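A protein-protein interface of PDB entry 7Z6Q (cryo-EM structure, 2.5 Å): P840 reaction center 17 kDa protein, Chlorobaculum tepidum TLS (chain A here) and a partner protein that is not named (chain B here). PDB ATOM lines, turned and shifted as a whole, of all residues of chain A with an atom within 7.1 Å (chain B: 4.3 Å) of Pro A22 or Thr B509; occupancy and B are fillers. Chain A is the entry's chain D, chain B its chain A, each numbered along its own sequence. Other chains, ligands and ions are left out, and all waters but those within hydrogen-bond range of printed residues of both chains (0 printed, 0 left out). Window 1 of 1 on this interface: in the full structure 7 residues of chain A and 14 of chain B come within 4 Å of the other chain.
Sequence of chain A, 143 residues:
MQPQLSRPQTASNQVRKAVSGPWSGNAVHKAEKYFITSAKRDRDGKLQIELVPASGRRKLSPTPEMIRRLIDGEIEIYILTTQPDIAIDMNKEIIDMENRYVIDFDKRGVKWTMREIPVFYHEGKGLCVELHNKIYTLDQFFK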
ATOM      1  N   SER A  20      23.290 -17.633   2.385  1.00  0.00           N
ATOM      2  CA  SER A  20      22.453 -18.810   2.213  1.00  0.00           C
ATOM      3  C   SER A  20      21.654 -18.678   0.919  1.00  0.00           C
ATOM      4  O   SER A  20      21.461 -17.577   0.396  1.00  0.00           O
ATOM      5  CB  SER A  20      21.518 -19.001   3.404  1.00  0.00           C
ATOM      6  OG  SER A  20      20.554 -17.966   3.472  1.00  0.00           O
ATOM      7  N   GLY A  21      21.184 -19.821   0.411  1.00  0.00           N
ATOM      8  CA  GLY A  21      20.422 -19.865  -0.852  1.00  0.00           C
ATOM      9  C   GLY A  21      19.004 -19.339  -0.717  1.00  0.00           C
ATOM     10  O   GLY A  21      18.527 -19.148   0.418  1.00  0.00           O
ATOM     11  N   PRO A  22      18.261 -19.157  -1.829  1.00  0.00           N
ATOM     12  CA  PRO A  22      16.892 -18.649  -1.767  1.00  0.00           C
ATOM     13  C   PRO A  22      15.999 -19.615  -0.976  1.00  0.00           C
ATOM     14  O   PRO A  22      15.154 -19.161  -0.238  1.00  0.00           O
ATOM     15  CB  PRO A  22      16.443 -18.626  -3.234  1.00  0.00           C
ATOM     16  CG  PRO A  22      17.732 -18.605  -4.020  1.00  0.00           C
ATOM     17  CD  PRO A  22      18.697 -19.430  -3.196  1.00  0.00           C
ATOM     18  N   TRP A  23      16.216 -20.918  -1.159  1.00  0.00           N
ATOM     19  CA  TRP A  23      15.416 -21.973  -0.485  1.00  0.00           C
ATOM     20  C   TRP A  23      15.572 -21.902   1.038  1.00  0.00           C
ATOM     21  O   TRP A  23      14.555 -22.099   1.724  1.00  0.00           O
ATOM     22  CB  TRP A  23      15.769 -23.338  -1.080  1.00  0.00           C
ATOM     23  CG  TRP A  23      15.791 -23.263  -2.575  1.00  0.00           C
ATOM     24  CD1 TRP A  23      14.777 -22.839  -3.382  1.00  0.00           C
ATOM     25  CD2 TRP A  23      16.897 -23.561  -3.444  1.00  0.00           C
ATOM     26  NE1 TRP A  23      15.166 -22.875  -4.693  1.00  0.00           N
ATOM     27  CE2 TRP A  23      16.461 -23.314  -4.762  1.00  0.00           C
ATOM     28  CE3 TRP A  23      18.201 -24.022  -3.241  1.00  0.00           C
ATOM     29  CZ2 TRP A  23      17.283 -23.517  -5.867  1.00  0.00           C
ATOM     30  CZ3 TRP A  23      19.014 -24.219  -4.336  1.00  0.00           C
ATOM     31  CH2 TRP A  23      18.559 -23.970  -5.630  1.00  0.00           C
ATOM     32  N   SER A  24      16.777 -21.638   1.553  1.00  0.00           N
ATOM     33  CA  SER A  24      16.934 -21.540   3.029  1.00  0.00           C
ATOM     34  C   SER A  24      16.327 -20.216   3.506  1.00  0.00           C
ATOM     35  O   SER A  24      16.727 -19.163   2.983  1.00  0.00           O
ATOM     36  CB  SER A  24      18.376 -21.652   3.435  1.00  0.00           C
ATOM     37  OG  SER A  24      18.953 -22.843   2.922  1.00  0.00           O
ATOM     38  N   GLY A  25      15.419 -20.274   4.485  1.00  0.00           N
ATOM     39  CA  GLY A  25      14.742 -19.068   5.003  1.00  0.00           C
ATOM     40  C   GLY A  25      13.868 -18.416   3.944  1.00  0.00           C
ATOM     41  O   GLY A  25      13.327 -19.140   3.091  1.00  0.00           O
ATOM     42  N   ASN A  26      13.689 -17.096   4.022  1.00  0.00           N
ATOM     43  CA  ASN A  26      12.882 -16.371   3.005  1.00  0.00           C
ATOM     44  C   ASN A  26      13.677 -16.323   1.696  1.00  0.00           C
ATOM     45  O   ASN A  26      14.915 -16.227   1.769  1.00  0.00           O
ATOM     46  CB  ASN A  26      12.472 -14.975   3.482  1.00  0.00           C
ATOM     47  CG  ASN A  26      11.150 -14.525   2.900  1.00  0.00           C
ATOM     48  OD1 ASN A  26      10.541 -15.240   2.111  1.00  0.00           O
ATOM     49  ND2 ASN A  26      10.698 -13.345   3.284  1.00  0.00           N
ATOM     50  N   ALA A  27      12.990 -16.383   0.551  1.00  0.00           N
ATOM     51  CA  ALA A  27      13.670 -16.356  -0.765  1.00  0.00           C
ATOM     52  C   ALA A  27      13.980 -14.911  -1.165  1.00  0.00           C
ATOM     53  O   ALA A  27      15.082 -14.659  -1.684  1.00  0.00           O
ATOM     54  CB  ALA A  27      12.816 -17.045  -1.797  1.00  0.00           C
ATOM     55  N   VAL A  28      13.036 -14.000  -0.924  1.00  0.00           N
ATOM     56  CA  VAL A  28      13.235 -12.563  -1.288  1.00  0.00           C
ATOM     57  C   VAL A  28      14.491 -11.990  -0.615  1.00  0.00           C
ATOM     58  O   VAL A  28      15.220 -11.239  -1.291  1.00  0.00           O
ATOM     59  CB  VAL A  28      11.982 -11.717  -0.985  1.00  0.00           C
ATOM     60  CG1 VAL A  28      10.837 -12.056  -1.923  1.00  0.00           C
ATOM     61  CG2 VAL A  28      11.534 -11.837   0.461  1.00  0.00           C
ATOM     62  N   HIS A  29      14.732 -12.338   0.653  1.00  0.00           N
ATOM     63  CA  HIS A  29      15.886 -11.815   1.434  1.00  0.00           C
ATOM     64  C   HIS A  29      17.220 -12.357   0.904  1.00  0.00           C
ATOM     65  O   HIS A  29      17.262 -13.528   0.497  1.00  0.00           O
ATOM     66  CB  HIS A  29      15.706 -12.144   2.923  1.00  0.00           C
ATOM     67  CG  HIS A  29      14.417 -11.674   3.507  1.00  0.00           C
ATOM     68  ND1 HIS A  29      13.586 -10.790   2.855  1.00  0.00           N
ATOM     69  CD2 HIS A  29      13.814 -11.961   4.681  1.00  0.00           C
ATOM     70  CE1 HIS A  29      12.526 -10.550   3.600  1.00  0.00           C
ATOM     71  NE2 HIS A  29      12.642 -11.255   4.726  1.00  0.00           N
ATOM     72  N   GLN B 418      21.678 -22.844  -7.587  1.00  0.00           N
ATOM     73  CA  GLN B 418      21.378 -21.822  -8.632  1.00  0.00           C
ATOM     74  C   GLN B 418      22.492 -21.765  -9.681  1.00  0.00           C
ATOM     75  O   GLN B 418      22.180 -21.485 -10.846  1.00  0.00           O
ATOM     76  CB  GLN B 418      21.064 -20.455  -8.027  1.00  0.00           C
ATOM     77  CG  GLN B 418      19.637 -20.344  -7.516  1.00  0.00           C
ATOM     78  CD  GLN B 418      19.098 -18.944  -7.655  1.00  0.00           C
ATOM     79  OE1 GLN B 418      19.845 -17.971  -7.651  1.00  0.00           O
ATOM     80  NE2 GLN B 418      17.787 -18.832  -7.780  1.00  0.00           N
ATOM     81  N   PHE B 505      13.399 -25.474 -12.785  1.00  0.00           N
ATOM     82  CA  PHE B 505      14.364 -24.757 -11.967  1.00  0.00           C
ATOM     83  C   PHE B 505      13.850 -23.446 -11.393  1.00  0.00           C
ATOM     84  O   PHE B 505      14.307 -23.049 -10.317  1.00  0.00           O
ATOM     85  CB  PHE B 505      15.636 -24.465 -12.779  1.00  0.00           C
ATOM     86  CG  PHE B 505      16.459 -25.686 -13.082  1.00  0.00           C
ATOM     87  CD1 PHE B 505      16.221 -26.883 -12.430  1.00  0.00           C
ATOM     88  CD2 PHE B 505      17.473 -25.634 -14.021  1.00  0.00           C
ATOM     89  CE1 PHE B 505      16.980 -28.001 -12.710  1.00  0.00           C
ATOM     90  CE2 PHE B 505      18.235 -26.748 -14.304  1.00  0.00           C
ATOM     91  CZ  PHE B 505      17.988 -27.933 -13.649  1.00  0.00           C
ATOM     92  N   PHE B 506      12.931 -22.773 -12.092  1.00  0.00           N
ATOM     93  CA  PHE B 506      12.474 -21.436 -11.626  1.00  0.00           C
ATOM     94  C   PHE B 506      10.999 -21.430 -11.213  1.00  0.00           C
ATOM     95  O   PHE B 506      10.319 -20.433 -11.487  1.00  0.00           O
ATOM     96  CB  PHE B 506      12.756 -20.363 -12.682  1.00  0.00           C
ATOM     97  CG  PHE B 506      14.135 -20.406 -13.291  1.00  0.00           C
ATOM     98  CD1 PHE B 506      15.261 -20.573 -12.503  1.00  0.00           C
ATOM     99  CD2 PHE B 506      14.312 -20.240 -14.653  1.00  0.00           C
ATOM    100  CE1 PHE B 506      16.527 -20.615 -13.065  1.00  0.00           C
ATOM    101  CE2 PHE B 506      15.578 -20.272 -15.215  1.00  0.00           C
ATOM    102  CZ  PHE B 506      16.683 -20.459 -14.420  1.00  0.00           C
ATOM    103  N   ALA B 507      10.518 -22.502 -10.585  1.00  0.00           N
ATOM    104  CA  ALA B 507       9.102 -22.546 -10.152  1.00  0.00           C
ATOM    105  C   ALA B 507       8.825 -21.476  -9.087  1.00  0.00           C
ATOM    106  O   ALA B 507       7.775 -20.817  -9.172  1.00  0.00           O
ATOM    107  CB  ALA B 507       8.767 -23.927  -9.646  1.00  0.00           C
ATOM    108  N   HIS B 508       9.729 -21.309  -8.116  1.00  0.00           N
ATOM    109  CA  HIS B 508       9.505 -20.310  -7.036  1.00  0.00           C
ATOM    110  C   HIS B 508      10.377 -19.067  -7.234  1.00  0.00           C
ATOM    111  O   HIS B 508       9.866 -17.947  -7.062  1.00  0.00           O
ATOM    112  CB  HIS B 508       9.755 -20.943  -5.665  1.00  0.00           C
ATOM    113  CG  HIS B 508       9.295 -20.101  -4.525  1.00  0.00           C
ATOM    114  ND1 HIS B 508      10.155 -19.653  -3.548  1.00  0.00           N
ATOM    115  CD2 HIS B 508       8.073 -19.626  -4.205  1.00  0.00           C
ATOM    116  CE1 HIS B 508       9.479 -18.941  -2.670  1.00  0.00           C
ATOM    117  NE2 HIS B 508       8.201 -18.909  -3.051  1.00  0.00           N
ATOM    118  N   THR B 509      11.649 -19.270  -7.572  1.00  0.00           N
ATOM    119  CA  THR B 509      12.590 -18.137  -7.737  1.00  0.00           C
ATOM    120  C   THR B 509      13.506 -18.391  -8.932  1.00  0.00           C
ATOM    121  O   THR B 509      13.677 -19.553  -9.315  1.00  0.00           O
ATOM    122  CB  THR B 509      13.465 -17.949  -6.489  1.00  0.00           C
ATOM    123  OG1 THR B 509      14.509 -18.924  -6.527  1.00  0.00           O
ATOM    124  CG2 THR B 509      12.699 -18.059  -5.190  1.00  0.00           C
ATOM    125  N   SER B 510      14.073 -17.317  -9.475  1.00  0.00           N
ATOM    126  CA  SER B 510      14.995 -17.367 -10.630  1.00  0.00           C
ATOM    127  C   SER B 510      16.219 -16.525 -10.272  1.00  0.00           C
ATOM    128  O   SER B 510      16.143 -15.731  -9.319  1.00  0.00           O
ATOM    129  CB  SER B 510      14.302 -16.834 -11.852  1.00  0.00           C
ATOM    130  OG  SER B 510      15.237 -16.455 -12.845  1.00  0.00           O
ATOM    131  N   ASP B 514      15.600 -13.440  -7.676  1.00  0.00           N
ATOM    132  CA  ASP B 514      16.425 -13.325  -6.479  1.00  0.00           C
ATOM    133  C   ASP B 514      17.235 -12.045  -6.502  1.00  0.00           C
ATOM    134  O   ASP B 514      17.503 -11.460  -5.447  1.00  0.00           O
ATOM    135  CB  ASP B 514      17.349 -14.530  -6.325  1.00  0.00           C
ATOM    136  CG  ASP B 514      18.195 -14.450  -5.085  1.00  0.00           C
ATOM    137  OD1 ASP B 514      17.618 -14.490  -3.978  1.00  0.00           O
ATOM    138  OD2 ASP B 514      19.436 -14.359  -5.200  1.00  0.00           O
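Of the 8 printed residues of chain B, 4 touch a printed residue of chain A. Printed residues of chain B that touch a printed residue of chain A: Gln B418, His B508, Thr B509 and Asp B514. Of the 10 printed residues of chain A, 3 touch a printed residue of chain B. Printed residues of chain A that touch a printed residue of chain B: Pro A22, Trp A23 and Ala A27. Among the printed residues, 6 pairs touch across the chains. Among the printed residues, no Asp or Glu carboxylate lies within 4 Å of a Lys or Arg side-chain nitrogen of the other chain.
Among the printed residues, merely in contact across the chains: Ala A27 with Thr B509 (3.5 Å), Pro A22 with Gln B418 (3.8 Å), Pro A22 with Thr B509 (3.8 Å), Trp A23 with Gln B418 (3.9 Å) and Ala A27 with His B508 (3.9 Å).
Pro A22 touches two residues of chain B. Of the printed residues of chain B, Trp A23 touches Gln B418 (3.9 Å). Of the printed residues of chain B, Ala A27 touches His B508, Thr B509 and Asp B514. Printed residues of chain A within 4 Å of Gln B418: Pro A22 (3.8 Å) and Trp A23 (3.9 Å). Printed residues of chain A within 4 Å of His B508: Ala A27 (3.9 Å). Thr B509 touches just these residues of chain A: Pro A22 and Ala A27. Printed residues of chain A within 4 Å of Asp B514: Ala A27 (3.4 Å). The nearest residue of chain A that does not touch Thr B509 is Trp A23 (4.4 Å).
O of Ala A27 sits close to OD1 of Asp B514.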
